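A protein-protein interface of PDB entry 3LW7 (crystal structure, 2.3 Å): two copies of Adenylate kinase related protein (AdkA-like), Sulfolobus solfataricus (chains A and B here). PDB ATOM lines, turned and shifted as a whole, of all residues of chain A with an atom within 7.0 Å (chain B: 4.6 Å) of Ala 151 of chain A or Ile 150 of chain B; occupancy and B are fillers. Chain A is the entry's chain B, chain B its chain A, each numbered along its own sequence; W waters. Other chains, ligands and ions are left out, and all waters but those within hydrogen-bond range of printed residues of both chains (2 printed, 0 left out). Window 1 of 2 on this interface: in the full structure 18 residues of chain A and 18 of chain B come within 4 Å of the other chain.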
ATOM      1  N   THR A   7      -9.701 -20.924 -26.375  1.00  0.00           N
ATOM      2  CA  THR A   7      -8.730 -19.980 -25.851  1.00  0.00           C
ATOM      3  C   THR A   7      -8.603 -20.178 -24.335  1.00  0.00           C
ATOM      4  O   THR A   7      -9.478 -20.786 -23.705  1.00  0.00           O
ATOM      5  CB  THR A   7      -9.094 -18.537 -26.255  1.00  0.00           C
ATOM      6  OG1 THR A   7      -8.012 -17.659 -25.912  1.00  0.00           O
ATOM      7  CG2 THR A   7     -10.348 -18.067 -25.570  1.00  0.00           C
ATOM      8  N   ALA A 107     -13.813 -20.063 -24.150  1.00  0.00           N
ATOM      9  CA  ALA A 107     -12.709 -19.773 -23.241  1.00  0.00           C
ATOM     10  C   ALA A 107     -12.710 -20.728 -22.046  1.00  0.00           C
ATOM     11  O   ALA A 107     -13.765 -21.031 -21.464  1.00  0.00           O
ATOM     12  CB  ALA A 107     -12.757 -18.297 -22.770  1.00  0.00           C
ATOM     13  N   HIS A 109     -11.507 -20.697 -18.382  1.00  0.00           N
ATOM     14  CA  HIS A 109     -11.000 -19.825 -17.323  1.00  0.00           C
ATOM     15  C   HIS A 109     -10.542 -20.557 -16.057  1.00  0.00           C
ATOM     16  O   HIS A 109     -11.234 -21.469 -15.565  1.00  0.00           O
ATOM     17  CB  HIS A 109     -12.047 -18.766 -16.941  1.00  0.00           C
ATOM     18  CG  HIS A 109     -11.569 -17.837 -15.875  1.00  0.00           C
ATOM     19  ND1 HIS A 109     -10.599 -16.885 -16.109  1.00  0.00           N
ATOM     20  CD2 HIS A 109     -11.879 -17.749 -14.557  1.00  0.00           C
ATOM     21  CE1 HIS A 109     -10.340 -16.240 -14.987  1.00  0.00           C
ATOM     22  NE2 HIS A 109     -11.102 -16.744 -14.031  1.00  0.00           N
ATOM     23  N   ILE A 146      -4.966 -12.069 -25.911  1.00  0.00           N
ATOM     24  CA  ILE A 146      -5.767 -13.208 -25.444  1.00  0.00           C
ATOM     25  C   ILE A 146      -6.968 -12.791 -24.589  1.00  0.00           C
ATOM     26  O   ILE A 146      -8.011 -13.439 -24.628  1.00  0.00           O
ATOM     27  CB  ILE A 146      -4.891 -14.259 -24.703  1.00  0.00           C
ATOM     28  CG1 ILE A 146      -5.018 -15.632 -25.353  1.00  0.00           C
ATOM     29  CG2 ILE A 146      -5.243 -14.348 -23.226  1.00  0.00           C
ATOM     30  CD1 ILE A 146      -4.171 -16.701 -24.686  1.00  0.00           C
ATOM     31  N   GLY A 147      -6.821 -11.706 -23.823  1.00  0.00           N
ATOM     32  CA  GLY A 147      -7.880 -11.220 -22.956  1.00  0.00           C
ATOM     33  C   GLY A 147      -9.087 -10.724 -23.727  1.00  0.00           C
ATOM     34  O   GLY A 147     -10.223 -10.841 -23.262  1.00  0.00           O
ATOM     35  N   GLU A 148      -8.844 -10.162 -24.898  1.00  0.00           N
ATOM     36  CA  GLU A 148      -9.934  -9.693 -25.766  1.00  0.00           C
ATOM     37  C   GLU A 148     -10.726 -10.864 -26.356  1.00  0.00           C
ATOM     38  O   GLU A 148     -11.925 -10.763 -26.541  1.00  0.00           O
ATOM     39  CB  GLU A 148      -9.398  -8.801 -26.880  1.00  0.00           C
ATOM     40  CG  GLU A 148      -8.325  -7.829 -26.435  1.00  0.00           C
ATOM     41  CD  GLU A 148      -7.977  -6.784 -27.491  1.00  0.00           C
ATOM     42  OE1 GLU A 148      -8.005  -7.097 -28.708  1.00  0.00           O
ATOM     43  OE2 GLU A 148      -7.670  -5.632 -27.106  1.00  0.00           O
ATOM     44  N   VAL A 149     -10.050 -11.976 -26.638  1.00  0.00           N
ATOM     45  CA  VAL A 149     -10.723 -13.170 -27.169  1.00  0.00           C
ATOM     46  C   VAL A 149     -11.618 -13.702 -26.077  1.00  0.00           C
ATOM     47  O   VAL A 149     -12.794 -13.968 -26.304  1.00  0.00           O
ATOM     48  CB  VAL A 149      -9.720 -14.257 -27.608  1.00  0.00           C
ATOM     49  CG1 VAL A 149     -10.450 -15.468 -28.216  1.00  0.00           C
ATOM     50  CG2 VAL A 149      -8.780 -13.688 -28.640  1.00  0.00           C
ATOM     51  N   ILE A 150     -11.082 -13.797 -24.862  1.00  0.00           N
ATOM     52  CA  ILE A 150     -11.888 -14.248 -23.728  1.00  0.00           C
ATOM     53  C   ILE A 150     -13.086 -13.334 -23.480  1.00  0.00           C
ATOM     54  O   ILE A 150     -14.212 -13.818 -23.281  1.00  0.00           O
ATOM     55  CB  ILE A 150     -11.029 -14.370 -22.452  1.00  0.00           C
ATOM     56  CG1 ILE A 150      -9.973 -15.458 -22.644  1.00  0.00           C
ATOM     57  CG2 ILE A 150     -11.901 -14.679 -21.218  1.00  0.00           C
ATOM     58  CD1 ILE A 150      -8.862 -15.431 -21.540  1.00  0.00           C
ATOM     59  N   ALA A 151     -12.864 -12.020 -23.524  1.00  0.00           N
ATOM     60  CA  ALA A 151     -13.924 -11.051 -23.226  1.00  0.00           C
ATOM     61  C   ALA A 151     -15.066 -11.147 -24.227  1.00  0.00           C
ATOM     62  O   ALA A 151     -16.199 -10.738 -23.916  1.00  0.00           O
ATOM     63  CB  ALA A 151     -13.366  -9.626 -23.222  1.00  0.00           C
ATOM     64  N   MET A 152     -14.765 -11.688 -25.415  1.00  0.00           N
ATOM     65  CA  MET A 152     -15.722 -11.745 -26.534  1.00  0.00           C
ATOM     66  C   MET A 152     -16.205 -13.161 -26.810  1.00  0.00           C
ATOM     67  O   MET A 152     -16.838 -13.405 -27.835  1.00  0.00           O
ATOM     68  CB  MET A 152     -15.095 -11.167 -27.825  1.00  0.00           C
ATOM     69  CG  MET A 152     -14.659  -9.680 -27.721  1.00  0.00           C
ATOM     70  SD  MET A 152     -16.025  -8.469 -27.511  1.00  0.00           S
ATOM     71  CE  MET A 152     -16.514  -8.380 -29.235  1.00  0.00           C
ATOM     72  N   ALA A 153     -15.894 -14.090 -25.901  1.00  0.00           N
ATOM     73  CA  ALA A 153     -16.224 -15.515 -26.059  1.00  0.00           C
ATOM     74  C   ALA A 153     -17.722 -15.778 -26.096  1.00  0.00           C
ATOM     75  O   ALA A 153     -18.496 -15.059 -25.462  1.00  0.00           O
ATOM     76  CB  ALA A 153     -15.606 -16.331 -24.922  1.00  0.00           C
ATOM     77  N   ASP A 154     -18.115 -16.816 -26.835  1.00  0.00           N
ATOM     78  CA  ASP A 154     -19.471 -17.313 -26.819  1.00  0.00           C
ATOM     79  C   ASP A 154     -19.778 -18.088 -25.547  1.00  0.00           C
ATOM     80  O   ASP A 154     -20.905 -18.069 -25.084  1.00  0.00           O
ATOM     81  CB  ASP A 154     -19.719 -18.199 -28.049  1.00  0.00           C
ATOM     82  CG  ASP A 154     -19.485 -17.438 -29.365  1.00  0.00           C
ATOM     83  OD1 ASP A 154     -18.455 -17.658 -30.041  1.00  0.00           O
ATOM     84  OD2 ASP A 154     -20.320 -16.571 -29.704  1.00  0.00           O
ATOM     85  N   ILE A 156     -17.728 -19.244 -21.704  1.00  0.00           N
ATOM     86  CA  ILE A 156     -16.597 -19.351 -20.791  1.00  0.00           C
ATOM     87  C   ILE A 156     -16.868 -20.492 -19.840  1.00  0.00           C
ATOM     88  O   ILE A 156     -17.869 -20.494 -19.137  1.00  0.00           O
ATOM     89  CB  ILE A 156     -16.343 -18.060 -19.970  1.00  0.00           C
ATOM     90  CG1 ILE A 156     -16.102 -16.859 -20.890  1.00  0.00           C
ATOM     91  CG2 ILE A 156     -15.114 -18.236 -19.071  1.00  0.00           C
ATOM     92  CD1 ILE A 156     -15.802 -15.531 -20.120  1.00  0.00           C
ATOM     93  N   THR B   7     -16.210  -6.257 -13.002  1.00  0.00           N
ATOM     94  CA  THR B   7     -15.871  -5.829 -14.335  1.00  0.00           C
ATOM     95  C   THR B   7     -16.819  -6.525 -15.304  1.00  0.00           C
ATOM     96  O   THR B   7     -17.482  -7.501 -14.944  1.00  0.00           O
ATOM     97  CB  THR B   7     -14.410  -6.141 -14.665  1.00  0.00           C
ATOM     98  OG1 THR B   7     -14.077  -5.568 -15.934  1.00  0.00           O
ATOM     99  CG2 THR B   7     -14.145  -7.671 -14.710  1.00  0.00           C
ATOM    100  N   MET B   9     -18.189  -6.298 -19.874  1.00  0.00           N
ATOM    101  CA  MET B   9     -18.393  -5.545 -21.103  1.00  0.00           C
ATOM    102  C   MET B   9     -19.718  -4.790 -21.050  1.00  0.00           C
ATOM    103  O   MET B   9     -20.579  -5.121 -20.231  1.00  0.00           O
ATOM    104  CB  MET B   9     -18.297  -6.490 -22.329  1.00  0.00           C
ATOM    105  CG  MET B   9     -16.893  -7.127 -22.492  1.00  0.00           C
ATOM    106  SD  MET B   9     -15.556  -5.974 -22.933  1.00  0.00           S
ATOM    107  CE  MET B   9     -15.961  -5.660 -24.674  1.00  0.00           C
ATOM    108  N   ALA B 107     -15.723 -10.979 -12.813  1.00  0.00           N
ATOM    109  CA  ALA B 107     -16.211 -10.592 -14.147  1.00  0.00           C
ATOM    110  C   ALA B 107     -17.597 -11.167 -14.405  1.00  0.00           C
ATOM    111  O   ALA B 107     -17.871 -12.322 -14.083  1.00  0.00           O
ATOM    112  CB  ALA B 107     -15.247 -11.056 -15.233  1.00  0.00           C
ATOM    113  N   HIS B 109     -19.864 -12.123 -17.448  1.00  0.00           N
ATOM    114  CA  HIS B 109     -19.765 -12.365 -18.875  1.00  0.00           C
ATOM    115  C   HIS B 109     -21.113 -12.549 -19.588  1.00  0.00           C
ATOM    116  O   HIS B 109     -22.017 -13.275 -19.095  1.00  0.00           O
ATOM    117  CB  HIS B 109     -18.906 -13.583 -19.134  1.00  0.00           C
ATOM    118  CG  HIS B 109     -18.778 -13.910 -20.582  1.00  0.00           C
ATOM    119  ND1 HIS B 109     -18.032 -13.142 -21.452  1.00  0.00           N
ATOM    120  CD2 HIS B 109     -19.314 -14.910 -21.324  1.00  0.00           C
ATOM    121  CE1 HIS B 109     -18.117 -13.651 -22.670  1.00  0.00           C
ATOM    122  NE2 HIS B 109     -18.882 -14.727 -22.619  1.00  0.00           N
ATOM    123  N   LEU B 142     -12.053  -2.512 -24.850  1.00  0.00           N
ATOM    124  CA  LEU B 142     -10.938  -3.461 -24.853  1.00  0.00           C
ATOM    125  C   LEU B 142      -9.581  -2.759 -24.862  1.00  0.00           C
ATOM    126  O   LEU B 142      -8.643  -3.215 -24.192  1.00  0.00           O
ATOM    127  CB  LEU B 142     -11.021  -4.438 -26.041  1.00  0.00           C
ATOM    128  CG  LEU B 142     -12.144  -5.478 -25.974  1.00  0.00           C
ATOM    129  CD1 LEU B 142     -12.357  -6.132 -27.342  1.00  0.00           C
ATOM    130  CD2 LEU B 142     -11.866  -6.499 -24.879  1.00  0.00           C
ATOM    131  N   ILE B 146      -9.876  -3.794 -20.494  1.00  0.00           N
ATOM    132  CA  ILE B 146     -10.877  -4.635 -19.832  1.00  0.00           C
ATOM    133  C   ILE B 146     -10.730  -6.166 -20.077  1.00  0.00           C
ATOM    134  O   ILE B 146     -11.042  -6.973 -19.197  1.00  0.00           O
ATOM    135  CB  ILE B 146     -12.312  -4.133 -20.153  1.00  0.00           C
ATOM    136  CG1 ILE B 146     -13.319  -4.656 -19.134  1.00  0.00           C
ATOM    137  CG2 ILE B 146     -12.706  -4.511 -21.571  1.00  0.00           C
ATOM    138  CD1 ILE B 146     -14.590  -3.822 -19.050  1.00  0.00           C
ATOM    139  N   GLY B 147     -10.226  -6.566 -21.244  1.00  0.00           N
ATOM    140  CA  GLY B 147     -10.032  -7.999 -21.522  1.00  0.00           C
ATOM    141  C   GLY B 147      -8.987  -8.604 -20.591  1.00  0.00           C
ATOM    142  O   GLY B 147      -9.112  -9.746 -20.145  1.00  0.00           O
ATOM    143  N   GLU B 148      -7.971  -7.809 -20.261  1.00  0.00           N
ATOM    144  CA  GLU B 148      -6.936  -8.229 -19.319  1.00  0.00           C
ATOM    145  C   GLU B 148      -7.477  -8.434 -17.913  1.00  0.00           C
ATOM    146  O   GLU B 148      -7.077  -9.363 -17.237  1.00  0.00           O
ATOM    147  CB  GLU B 148      -5.760  -7.250 -19.355  1.00  0.00           C
ATOM    148  CG  GLU B 148      -5.180  -7.074 -20.772  1.00  0.00           C
ATOM    149  CD  GLU B 148      -3.797  -6.416 -20.791  1.00  0.00           C
ATOM    150  OE1 GLU B 148      -3.413  -5.773 -19.789  1.00  0.00           O
ATOM    151  OE2 GLU B 148      -3.081  -6.542 -21.822  1.00  0.00           O
ATOM    152  N   VAL B 149      -8.407  -7.583 -17.482  1.00  0.00           N
ATOM    153  CA  VAL B 149      -9.043  -7.762 -16.178  1.00  0.00           C
ATOM    154  C   VAL B 149      -9.891  -9.041 -16.140  1.00  0.00           C
ATOM    155  O   VAL B 149      -9.765  -9.863 -15.215  1.00  0.00           O
ATOM    156  CB  VAL B 149      -9.902  -6.543 -15.798  1.00  0.00           C
ATOM    157  CG1 VAL B 149     -10.441  -6.671 -14.370  1.00  0.00           C
ATOM    158  CG2 VAL B 149      -9.067  -5.288 -15.920  1.00  0.00           C
ATOM    159  N   ILE B 150     -10.725  -9.225 -17.159  1.00  0.00           N
ATOM    160  CA  ILE B 150     -11.523 -10.450 -17.291  1.00  0.00           C
ATOM    161  C   ILE B 150     -10.655 -11.720 -17.288  1.00  0.00           C
ATOM    162  O   ILE B 150     -10.946 -12.679 -16.579  1.00  0.00           O
ATOM    163  CB  ILE B 150     -12.460 -10.378 -18.552  1.00  0.00           C
ATOM    164  CG1 ILE B 150     -13.417  -9.177 -18.420  1.00  0.00           C
ATOM    165  CG2 ILE B 150     -13.239 -11.682 -18.715  1.00  0.00           C
ATOM    166  CD1 ILE B 150     -14.232  -8.869 -19.659  1.00  0.00           C
ATOM    167  N   ALA B 151      -9.589 -11.728 -18.081  1.00  0.00           N
ATOM    168  CA  ALA B 151      -8.726 -12.904 -18.185  1.00  0.00           C
ATOM    169  C   ALA B 151      -8.020 -13.243 -16.869  1.00  0.00           C
ATOM    170  O   ALA B 151      -7.666 -14.386 -16.633  1.00  0.00           O
ATOM    171  CB  ALA B 151      -7.702 -12.721 -19.314  1.00  0.00           C
ATOM    172  N   MET B 152      -7.833 -12.253 -16.009  1.00  0.00           N
ATOM    173  CA  MET B 152      -7.149 -12.448 -14.730  1.00  0.00           C
ATOM    174  C   MET B 152      -8.110 -12.491 -13.530  1.00  0.00           C
ATOM    175  O   MET B 152      -7.692 -12.367 -12.374  1.00  0.00           O
ATOM    176  CB  MET B 152      -6.105 -11.331 -14.553  1.00  0.00           C
ATOM    177  CG  MET B 152      -5.030 -11.322 -15.678  1.00  0.00           C
ATOM    178  SD  MET B 152      -3.945 -12.788 -15.717  1.00  0.00           S
ATOM    179  CE  MET B 152      -2.967 -12.416 -14.273  1.00  0.00           C
ATOM    180  N   ALA B 153      -9.398 -12.670 -13.806  1.00  0.00           N
ATOM    181  CA  ALA B 153     -10.428 -12.630 -12.780  1.00  0.00           C
ATOM    182  C   ALA B 153     -10.353 -13.790 -11.812  1.00  0.00           C
ATOM    183  O   ALA B 153      -9.985 -14.901 -12.189  1.00  0.00           O
ATOM    184  CB  ALA B 153     -11.813 -12.601 -13.434  1.00  0.00           C
ATOM    185  N   ILE B 156     -15.612 -15.673 -12.805  1.00  0.00           N
ATOM    186  CA  ILE B 156     -16.362 -15.219 -13.952  1.00  0.00           C
ATOM    187  C   ILE B 156     -17.770 -15.784 -13.860  1.00  0.00           C
ATOM    188  O   ILE B 156     -17.959 -17.010 -13.756  1.00  0.00           O
ATOM    189  CB  ILE B 156     -15.675 -15.609 -15.293  1.00  0.00           C
ATOM    190  CG1 ILE B 156     -14.390 -14.784 -15.452  1.00  0.00           C
ATOM    191  CG2 ILE B 156     -16.626 -15.343 -16.440  1.00  0.00           C
ATOM    192  CD1 ILE B 156     -13.534 -15.061 -16.698  1.00  0.00           C
HETATM  193  O   HOH W   1      -8.790 -16.519 -18.156  1.00  0.00           O
HETATM  194  O   HOH W   2     -16.946 -10.600 -21.397  1.00  0.00           O
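The backbone carbonyl oxygen (O) of Gly 147 of chain A lies close to the backbone carbonyl oxygen (O) of Gly 147 of chain B, at 3.5 Å. The backbone carbonyl oxygen (O) of Ala 153 of chain B sits at hydrogen-bond distance from a ring nitrogen (NE2) of His 109 of chain A (2.8 Å). The backbone carbonyl oxygen (O) of Ala 153 of chain A sits at hydrogen-bond distance from a ring nitrogen (NE2) of His 109 of chain B.
His 109 of chain A touches Ile 150 of chain B (CE1 to O, 3.9 Å). His 109 of chain A touches Ala 151 of chain B (CE1 to O, 3.6 Å). Gly 147 of chain A touches Ala 151 of chain B (CA to CB, 3.9 Å). Ile 150 of chain A touches His 109 of chain B. Ile 150 of chain A touches Ala 151 of chain B. Ala 151 of chain A touches His 109 of chain B (O to CE1, 3.7 Å). CB of Ala 151 of chain A touches CD2 of Leu 142 of chain B, at 3.8 Å. CB of Ala 151 of chain A touches CD1 of Ile 150 of chain B (3.7 Å). Met 152 of chain A touches Met 9 of chain B (SD to CE, 3.99 Å). His 109 of chain B touches Ile 156 of chain A.
Of the printed residues of chain B, His 109 of chain A touches Ile 150 (3.9 Å), Ala 151 (3.6 Å), Ala 153 (2.8 Å) and Ile 156 (3.5 Å). Ile 146 of chain A touches none of the printed residues of chain B. Ala 151 of chain A touches just these residues of chain B: Met 9, His 109, Leu 142 and Ile 150. Asp 154 of chain A touches none of the printed residues of chain B. Of the printed residues of chain B, Ile 156 of chain A touches His 109 (3.4 Å) and Ile 156 (3.8 Å). Of the printed residues of chain A, Met 9 of chain B touches Ala 151 (3.9 Å) and Met 152 (3.99 Å). Of the printed residues of chain A, His 109 of chain B touches Ile 150, Ala 151, Ala 153 and Ile 156. Ile 150 of chain B touches two residues of chain A. The nearest residue of chain A that does not touch Ile 150 of chain B is Ile 150 of chain A (4.1 Å). The nearest printed residue of chain B that does not touch Ile 150 of chain A is Ile 150 of chain B (4.1 Å).
Printed residues of chain A that touch a printed residue of chain B: His 109, Gly 147, Glu 148, Ile 150, Ala 151, Met 152, Ala 153 and Ile 156. Hydrophobic or aromatic side chains of chain A within 4 Å of the printed part of chain B: His 109, Ile 150, Ala 151, Met 152 and Ile 156. Among the printed residues, 17 pairs touch across the chains.
His 109 of chain A touches Ile 150 of chain B, and with the chains exchanged Ile 150 of chain A touches His 109 of chain B. His 109 of chain A touches Ala 151 of chain B, and with the chains exchanged Ala 151 of chain A touches His 109 of chain B. His 109 of chain A touches Ile 156 of chain B, and with the chains exchanged Ile 156 of chain A touches His 109 of chain B. Gly 147 of chain A touches Ala 151 of chain B, but with the chains exchanged Ala 151 of chain A does not touch Gly 147 of chain B (4.1 Å).
Water W2 bridges the backbone carbonyl oxygen (O) of Ala 151 of chain A (2.6 Å) and a ring nitrogen (ND1) of His 109 of chain B (2.8 Å). Water W1 bridges ND1 of His 109 of chain A (2.8 Å) and O of Ala 151 of chain B (2.9 Å).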
